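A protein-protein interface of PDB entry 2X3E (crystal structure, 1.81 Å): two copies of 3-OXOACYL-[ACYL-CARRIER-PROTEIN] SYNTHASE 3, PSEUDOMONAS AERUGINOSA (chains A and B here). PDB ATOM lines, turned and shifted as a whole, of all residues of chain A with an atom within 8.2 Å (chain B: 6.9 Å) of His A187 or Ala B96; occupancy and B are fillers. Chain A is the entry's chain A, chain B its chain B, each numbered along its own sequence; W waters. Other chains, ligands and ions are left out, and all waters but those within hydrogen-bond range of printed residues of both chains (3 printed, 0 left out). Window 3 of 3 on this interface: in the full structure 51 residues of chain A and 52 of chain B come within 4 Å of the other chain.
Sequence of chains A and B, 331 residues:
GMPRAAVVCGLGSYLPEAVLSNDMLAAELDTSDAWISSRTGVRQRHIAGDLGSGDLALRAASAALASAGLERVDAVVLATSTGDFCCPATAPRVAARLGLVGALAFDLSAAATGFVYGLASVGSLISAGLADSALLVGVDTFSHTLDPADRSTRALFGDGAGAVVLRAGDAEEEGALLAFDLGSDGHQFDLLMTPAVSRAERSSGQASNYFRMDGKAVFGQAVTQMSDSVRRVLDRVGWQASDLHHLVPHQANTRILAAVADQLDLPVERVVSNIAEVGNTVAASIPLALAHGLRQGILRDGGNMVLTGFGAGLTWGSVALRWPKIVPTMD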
ATOM      1  N   SER A 184      23.176  22.681   1.174  1.00  0.00           N
ATOM      2  CA  SER A 184      22.805  23.988   0.667  1.00  0.00           C
ATOM      3  C   SER A 184      23.103  25.051   1.714  1.00  0.00           C
ATOM      4  O   SER A 184      23.195  24.755   2.907  1.00  0.00           O
ATOM      5  CB  SER A 184      21.317  24.018   0.288  1.00  0.00           C
ATOM      6  OG  SER A 184      20.477  24.025   1.434  1.00  0.00           O
ATOM      7  N   ASP A 185      23.272  26.286   1.253  1.00  0.00           N
ATOM      8  CA  ASP A 185      23.380  27.437   2.136  1.00  0.00           C
ATOM      9  C   ASP A 185      22.562  28.568   1.526  1.00  0.00           C
ATOM     10  O   ASP A 185      23.078  29.378   0.760  1.00  0.00           O
ATOM     11  CB  ASP A 185      24.842  27.866   2.331  1.00  0.00           C
ATOM     12  CG  ASP A 185      24.975  29.072   3.240  1.00  0.00           C
ATOM     13  OD1 ASP A 185      23.947  29.504   3.804  1.00  0.00           O
ATOM     14  OD2 ASP A 185      26.101  29.593   3.398  1.00  0.00           O
ATOM     15  N   GLY A 186      21.277  28.598   1.872  1.00  0.00           N
ATOM     16  CA  GLY A 186      20.379  29.646   1.422  1.00  0.00           C
ATOM     17  C   GLY A 186      20.654  31.022   1.994  1.00  0.00           C
ATOM     18  O   GLY A 186      20.055  32.002   1.558  1.00  0.00           O
ATOM     19  N   HIS A 187      21.541  31.118   2.981  1.00  0.00           N
ATOM     20  CA  HIS A 187      21.900  32.428   3.534  1.00  0.00           C
ATOM     21  C   HIS A 187      22.679  33.248   2.500  1.00  0.00           C
ATOM     22  O   HIS A 187      22.653  34.478   2.528  1.00  0.00           O
ATOM     23  CB  HIS A 187      22.723  32.276   4.817  1.00  0.00           C
ATOM     24  CG  HIS A 187      22.025  31.514   5.903  1.00  0.00           C
ATOM     25  ND1 HIS A 187      20.945  32.021   6.591  1.00  0.00           N
ATOM     26  CD2 HIS A 187      22.269  30.292   6.437  1.00  0.00           C
ATOM     27  CE1 HIS A 187      20.549  31.144   7.497  1.00  0.00           C
ATOM     28  NE2 HIS A 187      21.329  30.082   7.419  1.00  0.00           N
ATOM     29  N   GLN A 188      23.373  32.558   1.597  1.00  0.00           N
ATOM     30  CA  GLN A 188      24.125  33.197   0.515  1.00  0.00           C
ATOM     31  C   GLN A 188      23.429  33.070  -0.845  1.00  0.00           C
ATOM     32  O   GLN A 188      24.085  33.059  -1.893  1.00  0.00           O
ATOM     33  CB  GLN A 188      25.518  32.580   0.436  1.00  0.00           C
ATOM     34  CG  GLN A 188      26.371  32.821   1.675  1.00  0.00           C
ATOM     35  CD  GLN A 188      27.769  32.249   1.509  1.00  0.00           C
ATOM     36  OE1 GLN A 188      28.688  32.958   1.114  1.00  0.00           O
ATOM     37  NE2 GLN A 188      27.919  30.947   1.763  1.00  0.00           N
ATOM     38  N   PHE A 189      22.100  32.996  -0.830  1.00  0.00           N
ATOM     39  CA  PHE A 189      21.310  32.796  -2.055  1.00  0.00           C
ATOM     40  C   PHE A 189      21.537  33.854  -3.146  1.00  0.00           C
ATOM     41  O   PHE A 189      21.253  33.602  -4.317  1.00  0.00           O
ATOM     42  CB  PHE A 189      19.815  32.786  -1.721  1.00  0.00           C
ATOM     43  CG  PHE A 189      19.240  34.160  -1.483  1.00  0.00           C
ATOM     44  CD1 PHE A 189      18.574  34.836  -2.505  1.00  0.00           C
ATOM     45  CD2 PHE A 189      19.376  34.785  -0.248  1.00  0.00           C
ATOM     46  CE1 PHE A 189      18.050  36.107  -2.296  1.00  0.00           C
ATOM     47  CE2 PHE A 189      18.845  36.049  -0.027  1.00  0.00           C
ATOM     48  CZ  PHE A 189      18.181  36.714  -1.058  1.00  0.00           C
ATOM     49  N   ASP A 190      22.025  35.029  -2.758  1.00  0.00           N
ATOM     50  CA  ASP A 190      22.144  36.171  -3.671  1.00  0.00           C
ATOM     51  C   ASP A 190      23.450  36.207  -4.477  1.00  0.00           C
ATOM     52  O   ASP A 190      23.614  37.061  -5.345  1.00  0.00           O
ATOM     53  CB  ASP A 190      22.007  37.480  -2.888  1.00  0.00           C
ATOM     54  CG  ASP A 190      23.049  37.617  -1.793  1.00  0.00           C
ATOM     55  OD1 ASP A 190      23.039  36.780  -0.857  1.00  0.00           O
ATOM     56  OD2 ASP A 190      23.871  38.556  -1.867  1.00  0.00           O
ATOM     57  N   LEU A 191      24.384  35.294  -4.198  1.00  0.00           N
ATOM     58  CA  LEU A 191      25.709  35.339  -4.860  1.00  0.00           C
ATOM     59  C   LEU A 191      25.691  35.047  -6.367  1.00  0.00           C
ATOM     60  O   LEU A 191      26.435  35.669  -7.129  1.00  0.00           O
ATOM     61  CB  LEU A 191      26.705  34.383  -4.186  1.00  0.00           C
ATOM     62  CG  LEU A 191      27.398  34.806  -2.890  1.00  0.00           C
ATOM     63  CD1 LEU A 191      28.501  33.803  -2.576  1.00  0.00           C
ATOM     64  CD2 LEU A 191      27.982  36.229  -2.974  1.00  0.00           C
ATOM     65  N   GLY A 313      22.236  28.843  -5.050  1.00  0.00           N
ATOM     66  CA  GLY A 313      21.362  28.339  -3.995  1.00  0.00           C
ATOM     67  C   GLY A 313      21.660  28.963  -2.636  1.00  0.00           C
ATOM     68  O   GLY A 313      20.774  29.560  -2.035  1.00  0.00           O
ATOM     69  N   LEU A 314      22.878  28.816  -2.112  1.00  0.00           N
ATOM     70  CA  LEU A 314      23.942  27.988  -2.674  1.00  0.00           C
ATOM     71  C   LEU A 314      23.625  26.508  -2.486  1.00  0.00           C
ATOM     72  O   LEU A 314      22.874  26.138  -1.578  1.00  0.00           O
ATOM     73  CB  LEU A 314      25.277  28.295  -1.982  1.00  0.00           C
ATOM     74  CG  LEU A 314      25.783  29.736  -2.085  1.00  0.00           C
ATOM     75  CD1 LEU A 314      27.088  29.923  -1.305  1.00  0.00           C
ATOM     76  CD2 LEU A 314      25.963  30.140  -3.536  1.00  0.00           C
ATOM     77  N   LEU B  58       7.845  29.497   3.400  1.00  0.00           N
ATOM     78  CA  LEU B  58       8.465  29.610   4.719  1.00  0.00           C
ATOM     79  C   LEU B  58       7.410  29.480   5.814  1.00  0.00           C
ATOM     80  O   LEU B  58       7.584  28.717   6.751  1.00  0.00           O
ATOM     81  CB  LEU B  58       9.201  30.941   4.864  1.00  0.00           C
ATOM     82  CG  LEU B  58       9.907  31.217   6.199  1.00  0.00           C
ATOM     83  CD1 LEU B  58      10.901  30.111   6.557  1.00  0.00           C
ATOM     84  CD2 LEU B  58      10.599  32.566   6.139  1.00  0.00           C
ATOM     85  N   VAL B  76      14.489  19.953   2.410  1.00  0.00           N
ATOM     86  CA  VAL B  76      13.342  20.770   2.005  1.00  0.00           C
ATOM     87  C   VAL B  76      13.214  20.712   0.487  1.00  0.00           C
ATOM     88  O   VAL B  76      14.151  21.061  -0.232  1.00  0.00           O
ATOM     89  CB  VAL B  76      13.487  22.253   2.417  1.00  0.00           C
ATOM     90  CG1 VAL B  76      12.272  23.052   1.948  1.00  0.00           C
ATOM     91  CG2 VAL B  76      13.659  22.391   3.925  1.00  0.00           C
ATOM     92  N   ALA B  91      14.046  26.659  -2.580  1.00  0.00           N
ATOM     93  CA  ALA B  91      14.143  25.760  -1.424  1.00  0.00           C
ATOM     94  C   ALA B  91      15.346  26.010  -0.495  1.00  0.00           C
ATOM     95  O   ALA B  91      15.186  25.993   0.729  1.00  0.00           O
ATOM     96  CB  ALA B  91      14.107  24.286  -1.881  1.00  0.00           C
ATOM     97  N   PRO B  92      16.550  26.246  -1.052  1.00  0.00           N
ATOM     98  CA  PRO B  92      17.684  26.513  -0.151  1.00  0.00           C
ATOM     99  C   PRO B  92      17.480  27.723   0.778  1.00  0.00           C
ATOM    100  O   PRO B  92      17.833  27.663   1.963  1.00  0.00           O
ATOM    101  CB  PRO B  92      18.844  26.760  -1.116  1.00  0.00           C
ATOM    102  CG  PRO B  92      18.470  25.983  -2.346  1.00  0.00           C
ATOM    103  CD  PRO B  92      16.986  26.156  -2.457  1.00  0.00           C
ATOM    104  N   ARG B  93      16.910  28.801   0.243  1.00  0.00           N
ATOM    105  CA  ARG B  93      16.634  30.001   1.034  1.00  0.00           C
ATOM    106  C   ARG B  93      15.608  29.707   2.128  1.00  0.00           C
ATOM    107  O   ARG B  93      15.781  30.119   3.274  1.00  0.00           O
ATOM    108  CB  ARG B  93      16.152  31.144   0.133  1.00  0.00           C
ATOM    109  CG  ARG B  93      15.805  32.403   0.894  1.00  0.00           C
ATOM    110  CD  ARG B  93      15.414  33.552  -0.003  1.00  0.00           C
ATOM    111  NE  ARG B  93      14.922  34.662   0.804  1.00  0.00           N
ATOM    112  CZ  ARG B  93      14.489  35.828   0.330  1.00  0.00           C
ATOM    113  NH1 ARG B  93      14.468  36.069  -0.981  1.00  0.00           N
ATOM    114  NH2 ARG B  93      14.068  36.761   1.183  1.00  0.00           N
ATOM    115  N   VAL B  94      14.550  28.989   1.769  1.00  0.00           N
ATOM    116  CA  VAL B  94      13.543  28.567   2.741  1.00  0.00           C
ATOM    117  C   VAL B  94      14.191  27.749   3.857  1.00  0.00           C
ATOM    118  O   VAL B  94      13.995  28.035   5.038  1.00  0.00           O
ATOM    119  CB  VAL B  94      12.423  27.761   2.072  1.00  0.00           C
ATOM    120  CG1 VAL B  94      11.447  27.201   3.123  1.00  0.00           C
ATOM    121  CG2 VAL B  94      11.690  28.631   1.056  1.00  0.00           C
ATOM    122  N   ALA B  95      14.996  26.761   3.479  1.00  0.00           N
ATOM    123  CA  ALA B  95      15.678  25.920   4.461  1.00  0.00           C
ATOM    124  C   ALA B  95      16.570  26.741   5.395  1.00  0.00           C
ATOM    125  O   ALA B  95      16.602  26.496   6.606  1.00  0.00           O
ATOM    126  CB  ALA B  95      16.492  24.836   3.758  1.00  0.00           C
ATOM    127  N   ALA B  96      17.281  27.720   4.835  1.00  0.00           N
ATOM    128  CA  ALA B  96      18.157  28.588   5.616  1.00  0.00           C
ATOM    129  C   ALA B  96      17.375  29.416   6.632  1.00  0.00           C
ATOM    130  O   ALA B  96      17.743  29.485   7.813  1.00  0.00           O
ATOM    131  CB  ALA B  96      18.956  29.509   4.691  1.00  0.00           C
ATOM    132  N   ARG B  97      16.292  30.044   6.174  1.00  0.00           N
ATOM    133  CA  ARG B  97      15.476  30.889   7.044  1.00  0.00           C
ATOM    134  C   ARG B  97      14.709  30.099   8.123  1.00  0.00           C
ATOM    135  O   ARG B  97      14.320  30.657   9.154  1.00  0.00           O
ATOM    136  CB  ARG B  97      14.526  31.746   6.204  1.00  0.00           C
ATOM    137  CG  ARG B  97      15.264  32.717   5.261  1.00  0.00           C
ATOM    138  CD  ARG B  97      14.315  33.739   4.664  1.00  0.00           C
ATOM    139  NE  ARG B  97      13.741  34.593   5.702  1.00  0.00           N
ATOM    140  CZ  ARG B  97      12.623  35.307   5.575  1.00  0.00           C
ATOM    141  NH1 ARG B  97      11.928  35.298   4.436  1.00  0.00           N
ATOM    142  NH2 ARG B  97      12.191  36.033   6.601  1.00  0.00           N
ATOM    143  N   LEU B  98      14.511  28.806   7.883  1.00  0.00           N
ATOM    144  CA  LEU B  98      13.992  27.880   8.898  1.00  0.00           C
ATOM    145  C   LEU B  98      15.033  27.462   9.946  1.00  0.00           C
ATOM    146  O   LEU B  98      14.698  26.780  10.921  1.00  0.00           O
ATOM    147  CB  LEU B  98      13.446  26.624   8.225  1.00  0.00           C
ATOM    148  CG  LEU B  98      12.143  26.775   7.444  1.00  0.00           C
ATOM    149  CD1 LEU B  98      11.936  25.549   6.592  1.00  0.00           C
ATOM    150  CD2 LEU B  98      10.965  26.991   8.393  1.00  0.00           C
ATOM    151  N   GLY B  99      16.289  27.840   9.729  1.00  0.00           N
ATOM    152  CA  GLY B  99      17.371  27.537  10.665  1.00  0.00           C
ATOM    153  C   GLY B  99      17.909  26.120  10.516  1.00  0.00           C
ATOM    154  O   GLY B  99      18.520  25.585  11.442  1.00  0.00           O
ATOM    155  N   LEU B 100      17.690  25.513   9.353  1.00  0.00           N
ATOM    156  CA  LEU B 100      18.110  24.133   9.113  1.00  0.00           C
ATOM    157  C   LEU B 100      19.608  24.057   8.871  1.00  0.00           C
ATOM    158  O   LEU B 100      20.248  25.059   8.536  1.00  0.00           O
ATOM    159  CB  LEU B 100      17.354  23.522   7.927  1.00  0.00           C
ATOM    160  CG  LEU B 100      15.821  23.490   7.998  1.00  0.00           C
ATOM    161  CD1 LEU B 100      15.263  22.679   6.841  1.00  0.00           C
ATOM    162  CD2 LEU B 100      15.307  22.943   9.334  1.00  0.00           C
ATOM    163  N   ALA B 103      20.736  22.012   4.607  1.00  0.00           N
ATOM    164  CA  ALA B 103      19.665  21.148   4.126  1.00  0.00           C
ATOM    165  C   ALA B 103      19.869  20.638   2.695  1.00  0.00           C
ATOM    166  O   ALA B 103      20.323  21.369   1.813  1.00  0.00           O
ATOM    167  CB  ALA B 103      18.302  21.873   4.234  1.00  0.00           C
HETATM  168  O   HOH W   1      20.018  26.296   3.000  1.00  0.00           O
HETATM  169  O   HOH W   2      17.612  29.745  -2.506  1.00  0.00           O
HETATM  170  O   HOH W   3      20.331  27.793   8.892  1.00  0.00           O
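The side-chain hydroxyl (OG) of Ser A184 lies within hydrogen-bond range of the backbone carbonyl oxygen (O) of Ala B103, 2.7 Å away.
N of His A187 lies within hydrogen-bond range of OD1 of Asp A185.
Among the printed residues, pairs that only touch across the chains: Ser A184 with Pro B92 (3.95 Å), Gly A186 with Pro B92 (3.3 Å), Gly A186 with Arg B93 (3.8 Å), Gly A186 with Ala B96 (3.5 Å), His A187 with Ala B96 (3.3 Å), Phe A189 with Arg B93 (3.8 Å) and Gly A313 with Pro B92 (3.5 Å).
His A187 touches one residue of chain B. Ala B96 touches just these residues of chain A: Gly A186 (3.5 Å) and His A187 (3.3 Å). No residue of chain A comes within 4 Å of Ala B95. Of the printed residues of chain A, Ala B103 touches Ser A184. Printed residues of chain B within 4 Å of Gly A313: Pro B92 (3.5 Å). Of the printed residues of chain B, Ser A184 touches Pro B92 and Ala B103. Of the printed residues of chain A, Pro B92 touches Ser A184 (3.95 Å), Gly A186 (3.3 Å) and Gly A313 (3.5 Å). Printed residues of chain B within 4 Å of Phe A189: Arg B93. Val B76 touches none of the printed residues of chain A. Arg B97 touches none of the printed residues of chain A. The nearest residue of chain B that does not touch His A187 is Arg B97 (4.6 Å). The nearest residue of chain A that does not touch Ala B96 is Asp A185 (4.9 Å). The nearest printed residue of chain A that does not touch Ala B103 is Asp A185 (5.8 Å).
Of the 13 printed residues of chain B, 4 touch a printed residue of chain A. Along chain B the printed residues that touch a printed residue of chain A span positions 92 to 103. Of the 10 printed residues of chain A, 5 touch a printed residue of chain B. Hydrophobic or aromatic side chains of chain A within 4 Å of the printed part of chain B: His A187 and Phe A189.
No position is printed for both chains. Of the 8 pairs that touch across the chains among the printed residues, none has its exchanged pair printed and touching as well.
Water W3 lies within hydrogen-bond range of O of Leu B100, NE2 of His A187 and O of Ala B96. Water W1 lies within hydrogen-bond range of the backbone carbonyl oxygen of Pro B92 (2.8 Å), the side-chain hydroxyl of Ser A184 (2.8 Å) and the backbone NH of Gly A186 (2.9 Å). Water W2 bridges N of Arg B93 (3.0 Å) and O of Gly A313 (3.2 Å).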
